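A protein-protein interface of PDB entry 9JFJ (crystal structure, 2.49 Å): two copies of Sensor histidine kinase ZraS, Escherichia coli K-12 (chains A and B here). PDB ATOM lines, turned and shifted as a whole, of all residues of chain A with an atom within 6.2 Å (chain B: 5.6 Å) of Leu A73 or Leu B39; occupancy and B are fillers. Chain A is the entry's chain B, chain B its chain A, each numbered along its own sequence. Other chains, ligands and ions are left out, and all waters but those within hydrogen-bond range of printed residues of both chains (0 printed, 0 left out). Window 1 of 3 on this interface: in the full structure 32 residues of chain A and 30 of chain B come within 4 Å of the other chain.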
ATOM      1  N   ILE A  35       2.216   4.698 -12.090  1.00  0.00           N
ATOM      2  CA  ILE A  35       2.816   3.399 -11.704  1.00  0.00           C
ATOM      3  C   ILE A  35       2.060   2.865 -10.495  1.00  0.00           C
ATOM      4  O   ILE A  35       1.883   1.658 -10.391  1.00  0.00           O
ATOM      5  CB  ILE A  35       4.313   3.596 -11.425  1.00  0.00           C
ATOM      6  CG1 ILE A  35       5.122   3.630 -12.722  1.00  0.00           C
ATOM      7  CG2 ILE A  35       4.842   2.560 -10.456  1.00  0.00           C
ATOM      8  CD1 ILE A  35       6.449   4.314 -12.583  1.00  0.00           C
ATOM      9  N   LEU A  39       0.021  -1.009  -9.200  1.00  0.00           N
ATOM     10  CA  LEU A  39       0.854  -1.751  -8.225  1.00  0.00           C
ATOM     11  C   LEU A  39      -0.028  -2.510  -7.265  1.00  0.00           C
ATOM     12  O   LEU A  39       0.201  -3.698  -7.065  1.00  0.00           O
ATOM     13  CB  LEU A  39       1.795  -0.811  -7.474  1.00  0.00           C
ATOM     14  CG  LEU A  39       3.080  -0.467  -8.206  1.00  0.00           C
ATOM     15  CD1 LEU A  39       4.080   0.149  -7.246  1.00  0.00           C
ATOM     16  CD2 LEU A  39       3.653  -1.713  -8.848  1.00  0.00           C
ATOM     17  N   LYS A  68       7.257  -8.902  -4.630  1.00  0.00           N
ATOM     18  CA  LYS A  68       8.442  -8.178  -4.134  1.00  0.00           C
ATOM     19  C   LYS A  68       8.813  -7.113  -5.149  1.00  0.00           C
ATOM     20  O   LYS A  68       9.206  -6.048  -4.737  1.00  0.00           O
ATOM     21  CB  LYS A  68       9.542  -9.172  -3.786  1.00  0.00           C
ATOM     22  CG  LYS A  68       9.288  -9.987  -2.526  1.00  0.00           C
ATOM     23  CD  LYS A  68      10.371 -10.996  -2.240  1.00  0.00           C
ATOM     24  CE  LYS A  68      10.083 -11.827  -1.008  1.00  0.00           C
ATOM     25  NZ  LYS A  68      10.037 -10.983   0.211  1.00  0.00           N
ATOM     26  N   GLU A  69       8.674  -7.422  -6.425  1.00  0.00           N
ATOM     27  CA  GLU A  69       8.994  -6.461  -7.499  1.00  0.00           C
ATOM     28  C   GLU A  69       8.070  -5.252  -7.452  1.00  0.00           C
ATOM     29  O   GLU A  69       8.567  -4.148  -7.606  1.00  0.00           O
ATOM     30  CB  GLU A  69       9.034  -7.164  -8.848  1.00  0.00           C
ATOM     31  CG  GLU A  69      10.193  -8.128  -8.982  1.00  0.00           C
ATOM     32  CD  GLU A  69      11.560  -7.513  -8.758  1.00  0.00           C
ATOM     33  OE1 GLU A  69      12.044  -7.551  -7.610  1.00  0.00           O
ATOM     34  OE2 GLU A  69      12.144  -7.009  -9.727  1.00  0.00           O
ATOM     35  N   ALA A  70       6.784  -5.457  -7.201  1.00  0.00           N
ATOM     36  CA  ALA A  70       5.883  -4.304  -7.037  1.00  0.00           C
ATOM     37  C   ALA A  70       6.316  -3.462  -5.832  1.00  0.00           C
ATOM     38  O   ALA A  70       6.436  -2.227  -5.969  1.00  0.00           O
ATOM     39  CB  ALA A  70       4.494  -4.828  -6.868  1.00  0.00           C
ATOM     40  N   ASP A  71       6.662  -4.119  -4.728  1.00  0.00           N
ATOM     41  CA  ASP A  71       7.142  -3.338  -3.563  1.00  0.00           C
ATOM     42  C   ASP A  71       8.416  -2.552  -3.911  1.00  0.00           C
ATOM     43  O   ASP A  71       8.538  -1.385  -3.489  1.00  0.00           O
ATOM     44  CB  ASP A  71       7.293  -4.232  -2.343  1.00  0.00           C
ATOM     45  CG  ASP A  71       5.991  -4.498  -1.611  1.00  0.00           C
ATOM     46  OD1 ASP A  71       4.995  -3.835  -1.945  1.00  0.00           O
ATOM     47  OD2 ASP A  71       5.991  -5.363  -0.720  1.00  0.00           O
ATOM     48  N   ARG A  72       9.332  -3.150  -4.662  1.00  0.00           N
ATOM     49  CA  ARG A  72      10.603  -2.494  -5.046  1.00  0.00           C
ATOM     50  C   ARG A  72      10.342  -1.319  -5.981  1.00  0.00           C
ATOM     51  O   ARG A  72      11.089  -0.357  -5.925  1.00  0.00           O
ATOM     52  CB  ARG A  72      11.585  -3.527  -5.598  1.00  0.00           C
ATOM     53  CG  ARG A  72      12.995  -3.012  -5.826  1.00  0.00           C
ATOM     54  CD  ARG A  72      13.950  -4.157  -6.070  1.00  0.00           C
ATOM     55  NE  ARG A  72      13.785  -4.809  -7.354  1.00  0.00           N
ATOM     56  CZ  ARG A  72      14.410  -4.432  -8.457  1.00  0.00           C
ATOM     57  NH1 ARG A  72      15.225  -3.394  -8.430  1.00  0.00           N
ATOM     58  NH2 ARG A  72      14.217  -5.085  -9.586  1.00  0.00           N
ATOM     59  N   LEU A  73       9.384  -1.450  -6.881  1.00  0.00           N
ATOM     60  CA  LEU A  73       9.025  -0.338  -7.782  1.00  0.00           C
ATOM     61  C   LEU A  73       8.470   0.799  -6.939  1.00  0.00           C
ATOM     62  O   LEU A  73       8.822   1.941  -7.199  1.00  0.00           O
ATOM     63  CB  LEU A  73       7.994  -0.858  -8.781  1.00  0.00           C
ATOM     64  CG  LEU A  73       7.500   0.106  -9.837  1.00  0.00           C
ATOM     65  CD1 LEU A  73       8.634   0.507 -10.764  1.00  0.00           C
ATOM     66  CD2 LEU A  73       6.392  -0.562 -10.612  1.00  0.00           C
ATOM     67  N   ASN A  74       7.679   0.463  -5.927  1.00  0.00           N
ATOM     68  CA  ASN A  74       7.207   1.551  -5.044  1.00  0.00           C
ATOM     69  C   ASN A  74       8.428   2.195  -4.415  1.00  0.00           C
ATOM     70  O   ASN A  74       8.517   3.412  -4.472  1.00  0.00           O
ATOM     71  CB  ASN A  74       6.215   1.083  -3.984  1.00  0.00           C
ATOM     72  CG  ASN A  74       5.613   2.226  -3.203  1.00  0.00           C
ATOM     73  OD1 ASN A  74       5.242   3.244  -3.776  1.00  0.00           O
ATOM     74  ND2 ASN A  74       5.514   2.064  -1.893  1.00  0.00           N
ATOM     75  N   ARG A  75       9.375   1.405  -3.933  1.00  0.00           N
ATOM     76  CA  ARG A  75      10.529   2.052  -3.273  1.00  0.00           C
ATOM     77  C   ARG A  75      11.258   2.955  -4.273  1.00  0.00           C
ATOM     78  O   ARG A  75      11.609   4.067  -3.898  1.00  0.00           O
ATOM     79  CB  ARG A  75      11.414   1.021  -2.577  1.00  0.00           C
ATOM     80  CG  ARG A  75      10.852   0.543  -1.247  1.00  0.00           C
ATOM     81  CD  ARG A  75      11.728  -0.465  -0.533  1.00  0.00           C
ATOM     82  NE  ARG A  75      11.333  -1.841  -0.803  1.00  0.00           N
ATOM     83  CZ  ARG A  75      11.972  -2.659  -1.620  1.00  0.00           C
ATOM     84  NH1 ARG A  75      13.066  -2.253  -2.242  1.00  0.00           N
ATOM     85  NH2 ARG A  75      11.525  -3.885  -1.802  1.00  0.00           N
ATOM     86  N   VAL A  76      11.449   2.510  -5.497  1.00  0.00           N
ATOM     87  CA  VAL A  76      12.229   3.327  -6.461  1.00  0.00           C
ATOM     88  C   VAL A  76      11.477   4.611  -6.825  1.00  0.00           C
ATOM     89  O   VAL A  76      12.122   5.665  -7.007  1.00  0.00           O
ATOM     90  CB  VAL A  76      12.727   2.514  -7.670  1.00  0.00           C
ATOM     91  CG1 VAL A  76      13.724   3.299  -8.501  1.00  0.00           C
ATOM     92  CG2 VAL A  76      13.369   1.211  -7.235  1.00  0.00           C
ATOM     93  N   VAL A  77      10.160   4.528  -6.977  1.00  0.00           N
ATOM     94  CA  VAL A  77       9.362   5.756  -7.275  1.00  0.00           C
ATOM     95  C   VAL A  77       9.422   6.710  -6.072  1.00  0.00           C
ATOM     96  O   VAL A  77       9.511   7.935  -6.283  1.00  0.00           O
ATOM     97  CB  VAL A  77       7.947   5.472  -7.819  1.00  0.00           C
ATOM     98  CG1 VAL A  77       7.991   4.703  -9.122  1.00  0.00           C
ATOM     99  CG2 VAL A  77       7.059   4.766  -6.821  1.00  0.00           C
ATOM    100  N   SER A  78       9.405   6.161  -4.861  1.00  0.00           N
ATOM    101  CA  SER A  78       9.539   7.002  -3.656  1.00  0.00           C
ATOM    102  C   SER A  78      10.887   7.694  -3.716  1.00  0.00           C
ATOM    103  O   SER A  78      10.936   8.882  -3.452  1.00  0.00           O
ATOM    104  CB  SER A  78       9.416   6.192  -2.411  1.00  0.00           C
ATOM    105  OG  SER A  78       8.152   5.559  -2.348  1.00  0.00           O
ATOM    106  N   ILE B  35      13.625   2.056 -12.189  1.00  0.00           N
ATOM    107  CA  ILE B  35      12.153   1.807 -12.239  1.00  0.00           C
ATOM    108  C   ILE B  35      11.877   0.855 -13.401  1.00  0.00           C
ATOM    109  O   ILE B  35      11.168  -0.165 -13.202  1.00  0.00           O
ATOM    110  CB  ILE B  35      11.419   3.150 -12.421  1.00  0.00           C
ATOM    111  CG1 ILE B  35      11.369   3.961 -11.122  1.00  0.00           C
ATOM    112  CG2 ILE B  35      10.031   2.950 -12.998  1.00  0.00           C
ATOM    113  CD1 ILE B  35      11.020   5.410 -11.324  1.00  0.00           C
ATOM    114  N   ARG B  36      12.560   1.016 -14.528  1.00  0.00           N
ATOM    115  CA  ARG B  36      12.377   0.109 -15.691  1.00  0.00           C
ATOM    116  C   ARG B  36      12.674  -1.349 -15.327  1.00  0.00           C
ATOM    117  O   ARG B  36      12.063  -2.230 -15.914  1.00  0.00           O
ATOM    118  CB  ARG B  36      13.201   0.578 -16.888  1.00  0.00           C
ATOM    119  CG  ARG B  36      12.895  -0.157 -18.180  1.00  0.00           C
ATOM    120  CD  ARG B  36      14.076  -0.158 -19.121  1.00  0.00           C
ATOM    121  NE  ARG B  36      14.446   1.171 -19.574  1.00  0.00           N
ATOM    122  CZ  ARG B  36      13.836   1.814 -20.557  1.00  0.00           C
ATOM    123  NH1 ARG B  36      12.813   1.256 -21.176  1.00  0.00           N
ATOM    124  NH2 ARG B  36      14.250   3.015 -20.917  1.00  0.00           N
ATOM    125  N   ASN B  37      13.585  -1.599 -14.399  1.00  0.00           N
ATOM    126  CA  ASN B  37      13.952  -3.005 -14.124  1.00  0.00           C
ATOM    127  C   ASN B  37      12.834  -3.790 -13.443  1.00  0.00           C
ATOM    128  O   ASN B  37      12.476  -4.827 -13.989  1.00  0.00           O
ATOM    129  CB  ASN B  37      15.305  -3.084 -13.411  1.00  0.00           C
ATOM    130  CG  ASN B  37      16.431  -2.451 -14.193  1.00  0.00           C
ATOM    131  OD1 ASN B  37      16.357  -2.328 -15.412  1.00  0.00           O
ATOM    132  ND2 ASN B  37      17.483  -2.048 -13.500  1.00  0.00           N
ATOM    133  N   PRO B  38      12.236  -3.376 -12.305  1.00  0.00           N
ATOM    134  CA  PRO B  38      11.094  -4.066 -11.738  1.00  0.00           C
ATOM    135  C   PRO B  38       9.854  -4.048 -12.638  1.00  0.00           C
ATOM    136  O   PRO B  38       9.135  -4.982 -12.599  1.00  0.00           O
ATOM    137  CB  PRO B  38      10.835  -3.389 -10.391  1.00  0.00           C
ATOM    138  CG  PRO B  38      11.590  -2.114 -10.466  1.00  0.00           C
ATOM    139  CD  PRO B  38      12.788  -2.530 -11.275  1.00  0.00           C
ATOM    140  N   LEU B  39       9.683  -3.012 -13.448  1.00  0.00           N
ATOM    141  CA  LEU B  39       8.528  -2.999 -14.369  1.00  0.00           C
ATOM    142  C   LEU B  39       8.707  -4.107 -15.398  1.00  0.00           C
ATOM    143  O   LEU B  39       7.730  -4.780 -15.700  1.00  0.00           O
ATOM    144  CB  LEU B  39       8.426  -1.640 -15.054  1.00  0.00           C
ATOM    145  CG  LEU B  39       7.448  -0.666 -14.411  1.00  0.00           C
ATOM    146  CD1 LEU B  39       7.515   0.683 -15.091  1.00  0.00           C
ATOM    147  CD2 LEU B  39       6.038  -1.229 -14.458  1.00  0.00           C
ATOM    148  N   SER B  40       9.920  -4.253 -15.931  1.00  0.00           N
ATOM    149  CA  SER B  40      10.172  -5.306 -16.936  1.00  0.00           C
ATOM    150  C   SER B  40      10.006  -6.673 -16.278  1.00  0.00           C
ATOM    151  O   SER B  40       9.470  -7.571 -16.914  1.00  0.00           O
ATOM    152  CB  SER B  40      11.502  -5.117 -17.565  1.00  0.00           C
ATOM    153  OG  SER B  40      11.563  -3.862 -18.216  1.00  0.00           O
ATOM    154  N   SER B  41      10.458  -6.806 -15.041  1.00  0.00           N
ATOM    155  CA  SER B  41      10.234  -8.062 -14.307  1.00  0.00           C
ATOM    156  C   SER B  41       8.736  -8.235 -14.191  1.00  0.00           C
ATOM    157  O   SER B  41       8.266  -9.330 -14.459  1.00  0.00           O
ATOM    158  CB  SER B  41      10.852  -8.021 -12.965  1.00  0.00           C
ATOM    159  OG  SER B  41      10.541  -9.192 -12.238  1.00  0.00           O
ATOM    160  N   ILE B  42       8.027  -7.186 -13.783  1.00  0.00           N
ATOM    161  CA  ILE B  42       6.565  -7.404 -13.582  1.00  0.00           C
ATOM    162  C   ILE B  42       5.931  -7.802 -14.913  1.00  0.00           C
ATOM    163  O   ILE B  42       5.147  -8.739 -14.922  1.00  0.00           O
ATOM    164  CB  ILE B  42       5.860  -6.191 -12.942  1.00  0.00           C
ATOM    165  CG1 ILE B  42       6.466  -5.819 -11.590  1.00  0.00           C
ATOM    166  CG2 ILE B  42       4.363  -6.415 -12.840  1.00  0.00           C
ATOM    167  CD1 ILE B  42       5.800  -6.509 -10.442  1.00  0.00           C
ATOM    168  N   LYS B  43       6.320  -7.153 -15.997  1.00  0.00           N
ATOM    169  CA  LYS B  43       5.699  -7.439 -17.305  1.00  0.00           C
ATOM    170  C   LYS B  43       5.960  -8.886 -17.680  1.00  0.00           C
ATOM    171  O   LYS B  43       5.021  -9.550 -18.110  1.00  0.00           O
ATOM    172  CB  LYS B  43       6.347  -6.604 -18.409  1.00  0.00           C
ATOM    173  CG  LYS B  43       5.900  -6.890 -19.830  1.00  0.00           C
ATOM    174  CD  LYS B  43       6.656  -6.053 -20.838  1.00  0.00           C
ATOM    175  CE  LYS B  43       6.305  -6.370 -22.269  1.00  0.00           C
ATOM    176  NZ  LYS B  43       7.147  -5.610 -23.220  1.00  0.00           N
ATOM    177  N   GLY B  44       7.179  -9.358 -17.499  1.00  0.00           N
ATOM    178  CA  GLY B  44       7.374 -10.773 -17.820  1.00  0.00           C
ATOM    179  C   GLY B  44       6.603 -11.711 -16.930  1.00  0.00           C
ATOM    180  O   GLY B  44       6.016 -12.633 -17.463  1.00  0.00           O
ATOM    181  N   ALA B  70       2.020  -2.770 -17.731  1.00  0.00           N
ATOM    182  CA  ALA B  70       3.477  -2.732 -17.509  1.00  0.00           C
ATOM    183  C   ALA B  70       4.197  -2.335 -18.786  1.00  0.00           C
ATOM    184  O   ALA B  70       5.135  -1.567 -18.705  1.00  0.00           O
ATOM    185  CB  ALA B  70       3.943  -4.044 -17.002  1.00  0.00           C
ATOM    186  N   LEU B  73       3.748   1.279 -19.135  1.00  0.00           N
ATOM    187  CA  LEU B  73       4.557   1.955 -18.109  1.00  0.00           C
ATOM    188  C   LEU B  73       6.027   1.998 -18.516  1.00  0.00           C
ATOM    189  O   LEU B  73       6.640   2.998 -18.263  1.00  0.00           O
ATOM    190  CB  LEU B  73       4.295   1.304 -16.753  1.00  0.00           C
ATOM    191  CG  LEU B  73       2.965   1.659 -16.091  1.00  0.00           C
ATOM    192  CD1 LEU B  73       2.813   0.938 -14.766  1.00  0.00           C
ATOM    193  CD2 LEU B  73       2.845   3.157 -15.894  1.00  0.00           C
ATOM    194  N   ASN B  74       6.554   0.938 -19.103  1.00  0.00           N
ATOM    195  CA  ASN B  74       7.952   0.984 -19.592  1.00  0.00           C
ATOM    196  C   ASN B  74       8.054   2.040 -20.680  1.00  0.00           C
ATOM    197  O   ASN B  74       8.980   2.843 -20.615  1.00  0.00           O
ATOM    198  CB  ASN B  74       8.458  -0.382 -20.043  1.00  0.00           C
ATOM    199  CG  ASN B  74       9.017  -1.213 -18.912  1.00  0.00           C
ATOM    200  OD1 ASN B  74       9.465  -0.677 -17.909  1.00  0.00           O
ATOM    201  ND2 ASN B  74       9.016  -2.522 -19.081  1.00  0.00           N
ATOM    202  N   VAL B  77       8.099   5.405 -18.929  1.00  0.00           N
ATOM    203  CA  VAL B  77       9.365   5.637 -18.196  1.00  0.00           C
ATOM    204  C   VAL B  77      10.493   5.965 -19.168  1.00  0.00           C
ATOM    205  O   VAL B  77      11.276   6.835 -18.866  1.00  0.00           O
ATOM    206  CB  VAL B  77       9.702   4.463 -17.273  1.00  0.00           C
ATOM    207  CG1 VAL B  77      11.109   4.557 -16.713  1.00  0.00           C
ATOM    208  CG2 VAL B  77       8.688   4.329 -16.150  1.00  0.00           C
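Hydrophobic or aromatic side chains of chain B that line the printed part of chain A: Ile B35, Pro B38, Leu B39, Ile B42 and Leu B73.
Of the 13 printed residues of chain A, 7 touch a printed residue of chain B.
Among the printed residues, 12 pairs touch across the chains.
NH2 of Arg A72 lies within salt-bridge range of OE2 of Glu A69 (2.8 Å).
Among the printed residues, pairs that only touch across the chains: Ile A35 with Ile B35, Ile A35 with Leu B73, Glu A69 with Pro B38, Glu A69 with Ser B41, Glu A69 with Ile B42, Ala A70 with Ile B42, Arg A72 with Pro B38, Leu A73 with Ile B35, Leu A73 with Pro B38, Leu A73 with Leu B39, Val A76 with Ile B35 and Val A77 with Ile B35.
Of chain B, only Ile B35, Pro B38 and Leu B39 come within 4 Å of Leu A73.
Leu B39 touches one residue of chain A.
Printed residues of chain B within 4 Å of Ala A70: Ile B42 (3.5 Å).
Of the printed residues of chain A, Ile B35 touches Ile A35 (3.9 Å), Leu A73 (3.6 Å), Val A76 (3.6 Å) and Val A77 (3.8 Å).
Printed residues of chain B within 4 Å of Val A76: Ile B35 (3.6 Å).
Leu A39 touches none of the printed residues of chain B.
Ala B70 touches none of the printed residues of chain A.
The nearest residue of chain B that does not touch Leu A73 is Ile B42 (5.3 Å).
The nearest residue of chain A that does not touch Leu B39 is Ile A35 (4.5 Å).
The nearest printed residue of chain A that does not touch Ser B41 is Arg A72 (5.6 Å).
Ile B35 touches its own counterpart, Ile A35.
Ile A35 touches Leu B73, and with the chains exchanged Leu A73 touches Ile B35.
Leu A73 touches Leu B39, but with the chains exchanged Leu A39 does not touch Leu B73 (6.5 Å).
Val A77 touches Ile B35, but with the chains exchanged Ile A35 does not touch Val B77 (4.2 Å).
Positions printed for both chains: 35, 39, 70, 73, 74 and 77.
Of the 12 pairs that touch across the chains among the printed residues, 3 have their exchanged pair printed and touching as well.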
